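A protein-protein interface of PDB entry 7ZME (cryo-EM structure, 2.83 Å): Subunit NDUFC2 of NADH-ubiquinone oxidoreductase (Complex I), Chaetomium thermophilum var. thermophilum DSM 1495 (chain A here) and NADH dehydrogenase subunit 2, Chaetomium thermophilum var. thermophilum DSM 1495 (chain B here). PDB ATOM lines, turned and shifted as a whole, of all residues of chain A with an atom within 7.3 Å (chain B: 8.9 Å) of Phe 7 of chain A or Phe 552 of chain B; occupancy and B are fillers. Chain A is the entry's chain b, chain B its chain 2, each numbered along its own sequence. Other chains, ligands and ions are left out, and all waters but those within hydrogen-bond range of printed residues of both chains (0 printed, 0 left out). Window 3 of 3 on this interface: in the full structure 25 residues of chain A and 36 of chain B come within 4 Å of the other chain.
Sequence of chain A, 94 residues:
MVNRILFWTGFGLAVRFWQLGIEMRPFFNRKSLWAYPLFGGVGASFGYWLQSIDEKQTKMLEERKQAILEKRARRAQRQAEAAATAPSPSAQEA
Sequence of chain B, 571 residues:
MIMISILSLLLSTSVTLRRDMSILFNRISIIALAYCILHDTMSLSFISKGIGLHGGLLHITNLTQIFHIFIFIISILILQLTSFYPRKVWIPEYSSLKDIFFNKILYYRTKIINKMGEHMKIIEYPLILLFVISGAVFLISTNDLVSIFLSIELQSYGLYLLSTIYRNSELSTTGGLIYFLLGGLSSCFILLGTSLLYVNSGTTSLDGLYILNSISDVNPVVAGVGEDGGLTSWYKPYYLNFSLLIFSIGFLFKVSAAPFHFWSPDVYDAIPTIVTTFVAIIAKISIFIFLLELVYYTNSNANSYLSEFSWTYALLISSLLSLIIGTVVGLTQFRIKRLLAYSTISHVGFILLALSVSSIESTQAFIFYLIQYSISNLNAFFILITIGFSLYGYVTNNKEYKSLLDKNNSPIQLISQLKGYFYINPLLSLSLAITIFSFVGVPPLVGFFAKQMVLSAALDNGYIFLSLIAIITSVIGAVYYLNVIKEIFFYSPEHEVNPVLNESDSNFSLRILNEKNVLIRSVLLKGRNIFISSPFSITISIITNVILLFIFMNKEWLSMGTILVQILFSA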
ATOM      1  N   MET A   1      32.241  22.518  -7.355  1.00  0.00           N
ATOM      2  CA  MET A   1      31.970  21.088  -7.279  1.00  0.00           C
ATOM      3  C   MET A   1      31.058  20.742  -6.108  1.00  0.00           C
ATOM      4  O   MET A   1      30.205  19.862  -6.218  1.00  0.00           O
ATOM      5  CB  MET A   1      33.278  20.302  -7.169  1.00  0.00           C
ATOM      6  CG  MET A   1      33.092  18.792  -7.146  1.00  0.00           C
ATOM      7  SD  MET A   1      32.365  18.145  -8.662  1.00  0.00           S
ATOM      8  CE  MET A   1      31.687  16.595  -8.073  1.00  0.00           C
ATOM      9  N   VAL A   2      31.238  21.435  -4.988  1.00  0.00           N
ATOM     10  CA  VAL A   2      30.483  21.168  -3.770  1.00  0.00           C
ATOM     11  C   VAL A   2      29.868  22.473  -3.278  1.00  0.00           C
ATOM     12  O   VAL A   2      30.529  23.519  -3.266  1.00  0.00           O
ATOM     13  CB  VAL A   2      31.359  20.515  -2.684  1.00  0.00           C
ATOM     14  CG1 VAL A   2      32.477  21.449  -2.234  1.00  0.00           C
ATOM     15  CG2 VAL A   2      30.504  20.091  -1.498  1.00  0.00           C
ATOM     16  N   ASN A   3      28.590  22.416  -2.918  1.00  0.00           N
ATOM     17  CA  ASN A   3      27.908  23.490  -2.213  1.00  0.00           C
ATOM     18  C   ASN A   3      27.463  22.962  -0.859  1.00  0.00           C
ATOM     19  O   ASN A   3      26.909  21.861  -0.774  1.00  0.00           O
ATOM     20  CB  ASN A   3      26.704  24.005  -3.005  1.00  0.00           C
ATOM     21  CG  ASN A   3      25.887  25.016  -2.227  1.00  0.00           C
ATOM     22  OD1 ASN A   3      26.430  25.815  -1.464  1.00  0.00           O
ATOM     23  ND2 ASN A   3      24.573  24.988  -2.417  1.00  0.00           N
ATOM     24  N   ARG A   4      27.718  23.736   0.197  1.00  0.00           N
ATOM     25  CA  ARG A   4      27.399  23.262   1.539  1.00  0.00           C
ATOM     26  C   ARG A   4      25.905  23.010   1.696  1.00  0.00           C
ATOM     27  O   ARG A   4      25.496  22.115   2.442  1.00  0.00           O
ATOM     28  CB  ARG A   4      27.890  24.257   2.590  1.00  0.00           C
ATOM     29  CG  ARG A   4      27.699  23.768   4.017  1.00  0.00           C
ATOM     30  CD  ARG A   4      28.538  24.540   5.009  1.00  0.00           C
ATOM     31  NE  ARG A   4      29.964  24.415   4.740  1.00  0.00           N
ATOM     32  CZ  ARG A   4      30.748  25.431   4.404  1.00  0.00           C
ATOM     33  NH1 ARG A   4      32.038  25.229   4.176  1.00  0.00           N
ATOM     34  NH2 ARG A   4      30.241  26.651   4.299  1.00  0.00           N
ATOM     35  N   ILE A   5      25.077  23.776   0.991  1.00  0.00           N
ATOM     36  CA  ILE A   5      23.637  23.587   1.123  1.00  0.00           C
ATOM     37  C   ILE A   5      23.163  22.434   0.252  1.00  0.00           C
ATOM     38  O   ILE A   5      22.309  21.643   0.663  1.00  0.00           O
ATOM     39  CB  ILE A   5      22.888  24.889   0.791  1.00  0.00           C
ATOM     40  CG1 ILE A   5      23.636  26.100   1.348  1.00  0.00           C
ATOM     41  CG2 ILE A   5      21.483  24.835   1.346  1.00  0.00           C
ATOM     42  CD1 ILE A   5      23.846  26.066   2.843  1.00  0.00           C
ATOM     43  N   LEU A   6      23.700  22.322  -0.962  1.00  0.00           N
ATOM     44  CA  LEU A   6      23.301  21.237  -1.851  1.00  0.00           C
ATOM     45  C   LEU A   6      23.740  19.883  -1.306  1.00  0.00           C
ATOM     46  O   LEU A   6      22.989  18.905  -1.389  1.00  0.00           O
ATOM     47  CB  LEU A   6      23.872  21.474  -3.249  1.00  0.00           C
ATOM     48  CG  LEU A   6      23.424  20.556  -4.388  1.00  0.00           C
ATOM     49  CD1 LEU A   6      23.276  21.357  -5.669  1.00  0.00           C
ATOM     50  CD2 LEU A   6      24.408  19.413  -4.592  1.00  0.00           C
ATOM     51  N   PHE A   7      24.952  19.804  -0.755  1.00  0.00           N
ATOM     52  CA  PHE A   7      25.429  18.540  -0.203  1.00  0.00           C
ATOM     53  C   PHE A   7      24.542  18.068   0.939  1.00  0.00           C
ATOM     54  O   PHE A   7      24.095  16.919   0.957  1.00  0.00           O
ATOM     55  CB  PHE A   7      26.877  18.677   0.272  1.00  0.00           C
ATOM     56  CG  PHE A   7      27.372  17.484   1.042  1.00  0.00           C
ATOM     57  CD1 PHE A   7      27.869  16.376   0.384  1.00  0.00           C
ATOM     58  CD2 PHE A   7      27.332  17.468   2.428  1.00  0.00           C
ATOM     59  CE1 PHE A   7      28.313  15.275   1.091  1.00  0.00           C
ATOM     60  CE2 PHE A   7      27.776  16.372   3.137  1.00  0.00           C
ATOM     61  CZ  PHE A   7      28.269  15.276   2.469  1.00  0.00           C
ATOM     62  N   TRP A   8      24.280  18.947   1.908  1.00  0.00           N
ATOM     63  CA  TRP A   8      23.533  18.528   3.086  1.00  0.00           C
ATOM     64  C   TRP A   8      22.065  18.302   2.763  1.00  0.00           C
ATOM     65  O   TRP A   8      21.404  17.498   3.428  1.00  0.00           O
ATOM     66  CB  TRP A   8      23.710  19.549   4.207  1.00  0.00           C
ATOM     67  CG  TRP A   8      25.066  19.461   4.846  1.00  0.00           C
ATOM     68  CD1 TRP A   8      26.107  20.319   4.677  1.00  0.00           C
ATOM     69  CD2 TRP A   8      25.533  18.434   5.730  1.00  0.00           C
ATOM     70  NE1 TRP A   8      27.190  19.900   5.407  1.00  0.00           N
ATOM     71  CE2 TRP A   8      26.862  18.744   6.064  1.00  0.00           C
ATOM     72  CE3 TRP A   8      24.952  17.286   6.275  1.00  0.00           C
ATOM     73  CZ2 TRP A   8      27.622  17.951   6.920  1.00  0.00           C
ATOM     74  CZ3 TRP A   8      25.707  16.499   7.121  1.00  0.00           C
ATOM     75  CH2 TRP A   8      27.026  16.835   7.436  1.00  0.00           C
ATOM     76  N   THR A   9      21.541  18.987   1.746  1.00  0.00           N
ATOM     77  CA  THR A   9      20.225  18.632   1.229  1.00  0.00           C
ATOM     78  C   THR A   9      20.246  17.242   0.614  1.00  0.00           C
ATOM     79  O   THR A   9      19.347  16.430   0.857  1.00  0.00           O
ATOM     80  CB  THR A   9      19.766  19.662   0.199  1.00  0.00           C
ATOM     81  OG1 THR A   9      19.767  20.965   0.791  1.00  0.00           O
ATOM     82  CG2 THR A   9      18.368  19.334  -0.294  1.00  0.00           C
ATOM     83  N   GLY A  10      21.273  16.945  -0.183  1.00  0.00           N
ATOM     84  CA  GLY A  10      21.419  15.606  -0.720  1.00  0.00           C
ATOM     85  C   GLY A  10      21.834  14.598   0.326  1.00  0.00           C
ATOM     86  O   GLY A  10      21.568  13.403   0.178  1.00  0.00           O
ATOM     87  N   PHE A  11      22.493  15.058   1.392  1.00  0.00           N
ATOM     88  CA  PHE A  11      22.831  14.170   2.499  1.00  0.00           C
ATOM     89  C   PHE A  11      21.576  13.634   3.174  1.00  0.00           C
ATOM     90  O   PHE A  11      21.492  12.440   3.483  1.00  0.00           O
ATOM     91  CB  PHE A  11      23.709  14.911   3.504  1.00  0.00           C
ATOM     92  CG  PHE A  11      24.147  14.076   4.670  1.00  0.00           C
ATOM     93  CD1 PHE A  11      25.297  13.320   4.598  1.00  0.00           C
ATOM     94  CD2 PHE A  11      23.421  14.069   5.846  1.00  0.00           C
ATOM     95  CE1 PHE A  11      25.708  12.563   5.671  1.00  0.00           C
ATOM     96  CE2 PHE A  11      23.828  13.310   6.921  1.00  0.00           C
ATOM     97  CZ  PHE A  11      24.971  12.556   6.834  1.00  0.00           C
ATOM     98  N   GLY A  12      20.592  14.503   3.414  1.00  0.00           N
ATOM     99  CA  GLY A  12      19.356  14.066   4.036  1.00  0.00           C
ATOM    100  C   GLY A  12      18.574  13.095   3.179  1.00  0.00           C
ATOM    101  O   GLY A  12      17.883  12.218   3.702  1.00  0.00           O
ATOM    102  N   LEU A  13      18.667  13.239   1.856  1.00  0.00           N
ATOM    103  CA  LEU A  13      18.016  12.292   0.959  1.00  0.00           C
ATOM    104  C   LEU A  13      18.617  10.901   1.097  1.00  0.00           C
ATOM    105  O   LEU A  13      17.892   9.900   1.089  1.00  0.00           O
ATOM    106  CB  LEU A  13      18.126  12.779  -0.485  1.00  0.00           C
ATOM    107  CG  LEU A  13      17.358  14.048  -0.852  1.00  0.00           C
ATOM    108  CD1 LEU A  13      17.675  14.448  -2.276  1.00  0.00           C
ATOM    109  CD2 LEU A  13      15.873  13.849  -0.667  1.00  0.00           C
ATOM    110  N   GLY A  43      18.320  18.441   6.335  1.00  0.00           N
ATOM    111  CA  GLY A  43      19.699  18.574   5.898  1.00  0.00           C
ATOM    112  C   GLY A  43      20.018  19.966   5.393  1.00  0.00           C
ATOM    113  O   GLY A  43      21.088  20.508   5.672  1.00  0.00           O
ATOM    114  N   ALA A  44      19.091  20.566   4.642  1.00  0.00           N
ATOM    115  CA  ALA A  44      19.272  21.943   4.203  1.00  0.00           C
ATOM    116  C   ALA A  44      19.333  22.895   5.389  1.00  0.00           C
ATOM    117  O   ALA A  44      20.150  23.823   5.409  1.00  0.00           O
ATOM    118  CB  ALA A  44      18.145  22.340   3.253  1.00  0.00           C
ATOM    119  N   GLY A  47      22.626  22.489   6.805  1.00  0.00           N
ATOM    120  CA  GLY A  47      23.627  23.114   5.952  1.00  0.00           C
ATOM    121  C   GLY A  47      23.670  24.624   6.086  1.00  0.00           C
ATOM    122  O   GLY A  47      24.744  25.228   6.031  1.00  0.00           O
ATOM    123  N   LEU A  50      25.607  25.177   9.320  1.00  0.00           N
ATOM    124  CA  LEU A  50      27.039  24.982   9.105  1.00  0.00           C
ATOM    125  C   LEU A  50      27.643  26.132   8.319  1.00  0.00           C
ATOM    126  O   LEU A  50      28.756  26.578   8.616  1.00  0.00           O
ATOM    127  CB  LEU A  50      27.302  23.669   8.374  1.00  0.00           C
ATOM    128  CG  LEU A  50      27.287  22.395   9.202  1.00  0.00           C
ATOM    129  CD1 LEU A  50      27.675  21.240   8.326  1.00  0.00           C
ATOM    130  CD2 LEU A  50      28.233  22.526  10.370  1.00  0.00           C
ATOM    131  N   PRO B 444      38.045   6.174   1.747  1.00  0.00           N
ATOM    132  CA  PRO B 444      38.042   7.546   2.254  1.00  0.00           C
ATOM    133  C   PRO B 444      37.159   7.719   3.483  1.00  0.00           C
ATOM    134  O   PRO B 444      36.464   8.726   3.601  1.00  0.00           O
ATOM    135  CB  PRO B 444      37.481   8.326   1.073  1.00  0.00           C
ATOM    136  CG  PRO B 444      36.465   7.390   0.511  1.00  0.00           C
ATOM    137  CD  PRO B 444      36.973   5.980   0.758  1.00  0.00           C
ATOM    138  N   PHE B 449      41.197   9.030   8.094  1.00  0.00           N
ATOM    139  CA  PHE B 449      41.676  10.389   8.303  1.00  0.00           C
ATOM    140  C   PHE B 449      42.072  10.612   9.752  1.00  0.00           C
ATOM    141  O   PHE B 449      43.030  11.338  10.037  1.00  0.00           O
ATOM    142  CB  PHE B 449      40.603  11.384   7.873  1.00  0.00           C
ATOM    143  CG  PHE B 449      40.422  11.463   6.392  1.00  0.00           C
ATOM    144  CD1 PHE B 449      41.327  12.150   5.609  1.00  0.00           C
ATOM    145  CD2 PHE B 449      39.354  10.835   5.777  1.00  0.00           C
ATOM    146  CE1 PHE B 449      41.164  12.220   4.246  1.00  0.00           C
ATOM    147  CE2 PHE B 449      39.190  10.903   4.416  1.00  0.00           C
ATOM    148  CZ  PHE B 449      40.094  11.595   3.650  1.00  0.00           C
ATOM    149  N   ASN B 545      26.510   7.405   7.076  1.00  0.00           N
ATOM    150  CA  ASN B 545      26.714   8.394   6.028  1.00  0.00           C
ATOM    151  C   ASN B 545      27.797   9.398   6.399  1.00  0.00           C
ATOM    152  O   ASN B 545      28.493   9.908   5.515  1.00  0.00           O
ATOM    153  CB  ASN B 545      25.396   9.103   5.728  1.00  0.00           C
ATOM    154  CG  ASN B 545      24.572   8.381   4.680  1.00  0.00           C
ATOM    155  OD1 ASN B 545      24.682   8.663   3.491  1.00  0.00           O
ATOM    156  ND2 ASN B 545      23.749   7.439   5.118  1.00  0.00           N
ATOM    157  N   VAL B 546      27.949   9.703   7.690  1.00  0.00           N
ATOM    158  CA  VAL B 546      29.045  10.562   8.132  1.00  0.00           C
ATOM    159  C   VAL B 546      30.385   9.892   7.873  1.00  0.00           C
ATOM    160  O   VAL B 546      31.332  10.525   7.393  1.00  0.00           O
ATOM    161  CB  VAL B 546      28.872  10.925   9.618  1.00  0.00           C
ATOM    162  CG1 VAL B 546      30.115  11.622  10.144  1.00  0.00           C
ATOM    163  CG2 VAL B 546      27.663  11.816   9.804  1.00  0.00           C
ATOM    164  N   ILE B 547      30.488   8.602   8.194  1.00  0.00           N
ATOM    165  CA  ILE B 547      31.725   7.860   7.971  1.00  0.00           C
ATOM    166  C   ILE B 547      32.062   7.814   6.487  1.00  0.00           C
ATOM    167  O   ILE B 547      33.214   8.022   6.089  1.00  0.00           O
ATOM    168  CB  ILE B 547      31.596   6.444   8.558  1.00  0.00           C
ATOM    169  CG1 ILE B 547      31.397   6.504  10.070  1.00  0.00           C
ATOM    170  CG2 ILE B 547      32.801   5.598   8.192  1.00  0.00           C
ATOM    171  CD1 ILE B 547      31.178   5.150  10.704  1.00  0.00           C
ATOM    172  N   LEU B 548      31.063   7.537   5.650  1.00  0.00           N
ATOM    173  CA  LEU B 548      31.294   7.388   4.217  1.00  0.00           C
ATOM    174  C   LEU B 548      31.710   8.705   3.575  1.00  0.00           C
ATOM    175  O   LEU B 548      32.712   8.765   2.854  1.00  0.00           O
ATOM    176  CB  LEU B 548      30.033   6.843   3.547  1.00  0.00           C
ATOM    177  CG  LEU B 548      30.218   5.997   2.292  1.00  0.00           C
ATOM    178  CD1 LEU B 548      31.133   4.817   2.558  1.00  0.00           C
ATOM    179  CD2 LEU B 548      28.871   5.526   1.792  1.00  0.00           C
ATOM    180  N   LEU B 549      30.954   9.771   3.829  1.00  0.00           N
ATOM    181  CA  LEU B 549      31.110  11.036   3.123  1.00  0.00           C
ATOM    182  C   LEU B 549      31.819  12.091   3.959  1.00  0.00           C
ATOM    183  O   LEU B 549      31.542  13.284   3.808  1.00  0.00           O
ATOM    184  CB  LEU B 549      29.749  11.556   2.669  1.00  0.00           C
ATOM    185  CG  LEU B 549      28.821  10.506   2.070  1.00  0.00           C
ATOM    186  CD1 LEU B 549      27.405  11.033   1.987  1.00  0.00           C
ATOM    187  CD2 LEU B 549      29.329  10.086   0.710  1.00  0.00           C
ATOM    188  N   PHE B 550      32.731  11.677   4.839  1.00  0.00           N
ATOM    189  CA  PHE B 550      33.481  12.645   5.629  1.00  0.00           C
ATOM    190  C   PHE B 550      34.330  13.554   4.749  1.00  0.00           C
ATOM    191  O   PHE B 550      34.559  14.716   5.099  1.00  0.00           O
ATOM    192  CB  PHE B 550      34.361  11.924   6.649  1.00  0.00           C
ATOM    193  CG  PHE B 550      35.348  12.825   7.332  1.00  0.00           C
ATOM    194  CD1 PHE B 550      34.920  13.792   8.222  1.00  0.00           C
ATOM    195  CD2 PHE B 550      36.699  12.718   7.068  1.00  0.00           C
ATOM    196  CE1 PHE B 550      35.822  14.624   8.841  1.00  0.00           C
ATOM    197  CE2 PHE B 550      37.602  13.550   7.683  1.00  0.00           C
ATOM    198  CZ  PHE B 550      37.162  14.504   8.570  1.00  0.00           C
ATOM    199  N   ILE B 551      34.791  13.053   3.602  1.00  0.00           N
ATOM    200  CA  ILE B 551      35.679  13.826   2.744  1.00  0.00           C
ATOM    201  C   ILE B 551      34.980  15.015   2.101  1.00  0.00           C
ATOM    202  O   ILE B 551      35.642  15.862   1.494  1.00  0.00           O
ATOM    203  CB  ILE B 551      36.297  12.900   1.673  1.00  0.00           C
ATOM    204  CG1 ILE B 551      37.579  13.506   1.100  1.00  0.00           C
ATOM    205  CG2 ILE B 551      35.310  12.637   0.564  1.00  0.00           C
ATOM    206  CD1 ILE B 551      38.424  12.525   0.329  1.00  0.00           C
ATOM    207  N   PHE B 552      33.673  15.154   2.284  1.00  0.00           N
ATOM    208  CA  PHE B 552      32.931  16.281   1.672  1.00  0.00           C
ATOM    209  C   PHE B 552      32.418  17.216   2.763  1.00  0.00           C
ATOM    210  O   PHE B 552      32.132  18.365   2.434  1.00  0.00           O
ATOM    211  CB  PHE B 552      31.766  15.765   0.831  1.00  0.00           C
ATOM    212  CG  PHE B 552      32.111  14.779  -0.254  1.00  0.00           C
ATOM    213  CD1 PHE B 552      32.825  15.173  -1.373  1.00  0.00           C
ATOM    214  CD2 PHE B 552      31.690  13.462  -0.174  1.00  0.00           C
ATOM    215  CE1 PHE B 552      33.130  14.267  -2.375  1.00  0.00           C
ATOM    216  CE2 PHE B 552      31.994  12.557  -1.176  1.00  0.00           C
ATOM    217  CZ  PHE B 552      32.713  12.961  -2.276  1.00  0.00           C
ATOM    218  N   MET B 553      32.309  16.740   4.004  1.00  0.00           N
ATOM    219  CA  MET B 553      31.769  17.527   5.138  1.00  0.00           C
ATOM    220  C   MET B 553      32.887  17.814   6.141  1.00  0.00           C
ATOM    221  O   MET B 553      32.566  18.204   7.274  1.00  0.00           O
ATOM    222  CB  MET B 553      30.718  16.669   5.840  1.00  0.00           C
ATOM    223  CG  MET B 553      31.312  15.409   6.435  1.00  0.00           C
ATOM    224  SD  MET B 553      30.179  14.408   7.413  1.00  0.00           S
ATOM    225  CE  MET B 553      29.008  13.903   6.155  1.00  0.00           C
ATOM    226  N   ASN B 554      34.143  17.636   5.763  1.00  0.00           N
ATOM    227  CA  ASN B 554      35.278  17.745   6.717  1.00  0.00           C
ATOM    228  C   ASN B 554      35.563  19.138   7.280  1.00  0.00           C
ATOM    229  O   ASN B 554      36.099  19.188   8.394  1.00  0.00           O
ATOM    230  CB  ASN B 554      36.571  17.205   6.091  1.00  0.00           C
ATOM    231  CG  ASN B 554      37.052  17.995   4.891  1.00  0.00           C
ATOM    232  OD1 ASN B 554      37.804  18.956   5.033  1.00  0.00           O
ATOM    233  ND2 ASN B 554      36.642  17.590   3.702  1.00  0.00           N
ATOM    234  N   LYS B 555      35.238  20.221   6.571  1.00  0.00           N
ATOM    235  CA  LYS B 555      35.753  21.558   6.976  1.00  0.00           C
ATOM    236  C   LYS B 555      35.358  22.057   8.366  1.00  0.00           C
ATOM    237  O   LYS B 555      36.276  22.285   9.140  1.00  0.00           O
ATOM    238  CB  LYS B 555      35.434  22.597   5.898  1.00  0.00           C
ATOM    239  CG  LYS B 555      36.179  23.916   6.030  1.00  0.00           C
ATOM    240  CD  LYS B 555      35.929  24.861   4.884  1.00  0.00           C
ATOM    241  CE  LYS B 555      36.605  26.200   5.075  1.00  0.00           C
ATOM    242  NZ  LYS B 555      38.038  26.044   5.413  1.00  0.00           N
ATOM    243  N   GLU B 556      34.083  22.104   8.731  1.00  0.00           N
ATOM    244  CA  GLU B 556      33.723  22.721  10.038  1.00  0.00           C
ATOM    245  C   GLU B 556      34.227  21.865  11.192  1.00  0.00           C
ATOM    246  O   GLU B 556      34.694  22.438  12.177  1.00  0.00           O
ATOM    247  CB  GLU B 556      32.227  23.012  10.137  1.00  0.00           C
ATOM    248  CG  GLU B 556      31.781  24.194   9.298  1.00  0.00           C
ATOM    249  CD  GLU B 556      31.678  23.923   7.808  1.00  0.00           C
ATOM    250  OE1 GLU B 556      30.702  23.276   7.397  1.00  0.00           O
ATOM    251  OE2 GLU B 556      32.577  24.351   7.069  1.00  0.00           O
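The guanidinium group of Arg 4 of chain A lies within salt-bridge range of the side-chain carboxylate of Glu 556 of chain B, 3.0 Å away.
Among the printed residues, pairs that only touch across the chains: Phe 11 of chain A with Asn 545 of chain B (3.5 Å), Phe 7 of chain A with Phe 552 of chain B (3.5 Å), Trp 8 of chain A with Met 553 of chain B (3.5 Å), Leu 50 of chain A with Glu 556 of chain B (3.6 Å), Phe 11 of chain A with Met 553 of chain B (3.6 Å) and Arg 4 of chain A with Lys 555 of chain B (3.97 Å).
Printed residues of chain B within 4 Å of Arg 4 of chain A: Lys 555 and Glu 556.
Printed residues of chain B within 4 Å of Phe 7 of chain A: Phe 552.
No residue of chain B comes within 4 Å of Gly 10 of chain A.
Gly 12 of chain A touches none of the printed residues of chain B.
Printed residues of chain B within 4 Å of Leu 50 of chain A: Glu 556.
Printed residues of chain A within 4 Å of Lys 555 of chain B: Arg 4 (3.97 Å).
Printed residues of chain A within 4 Å of Glu 556 of chain B: Arg 4 (3.0 Å) and Leu 50 (3.6 Å).
The nearest residue of chain A that does not touch Phe 552 of chain B is Val 2 of chain A (4.6 Å).
The nearest printed residue of chain A that does not touch Glu 556 of chain B is Trp 8 of chain A (5.3 Å).
Hydrophobic or aromatic side chains of chain A that line the printed part of chain B: Phe 7, Trp 8, Phe 11 and Leu 50.
Of the 14 printed residues of chain B, 5 touch a printed residue of chain A.
Among the printed residues, 7 pairs touch across the chains.
Among the printed residues, Asp or Glu carboxylates within 4 Å of a Lys or Arg side-chain nitrogen of the other chain: Arg 4 of chain A with Glu 556 of chain B (3.0 Å).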
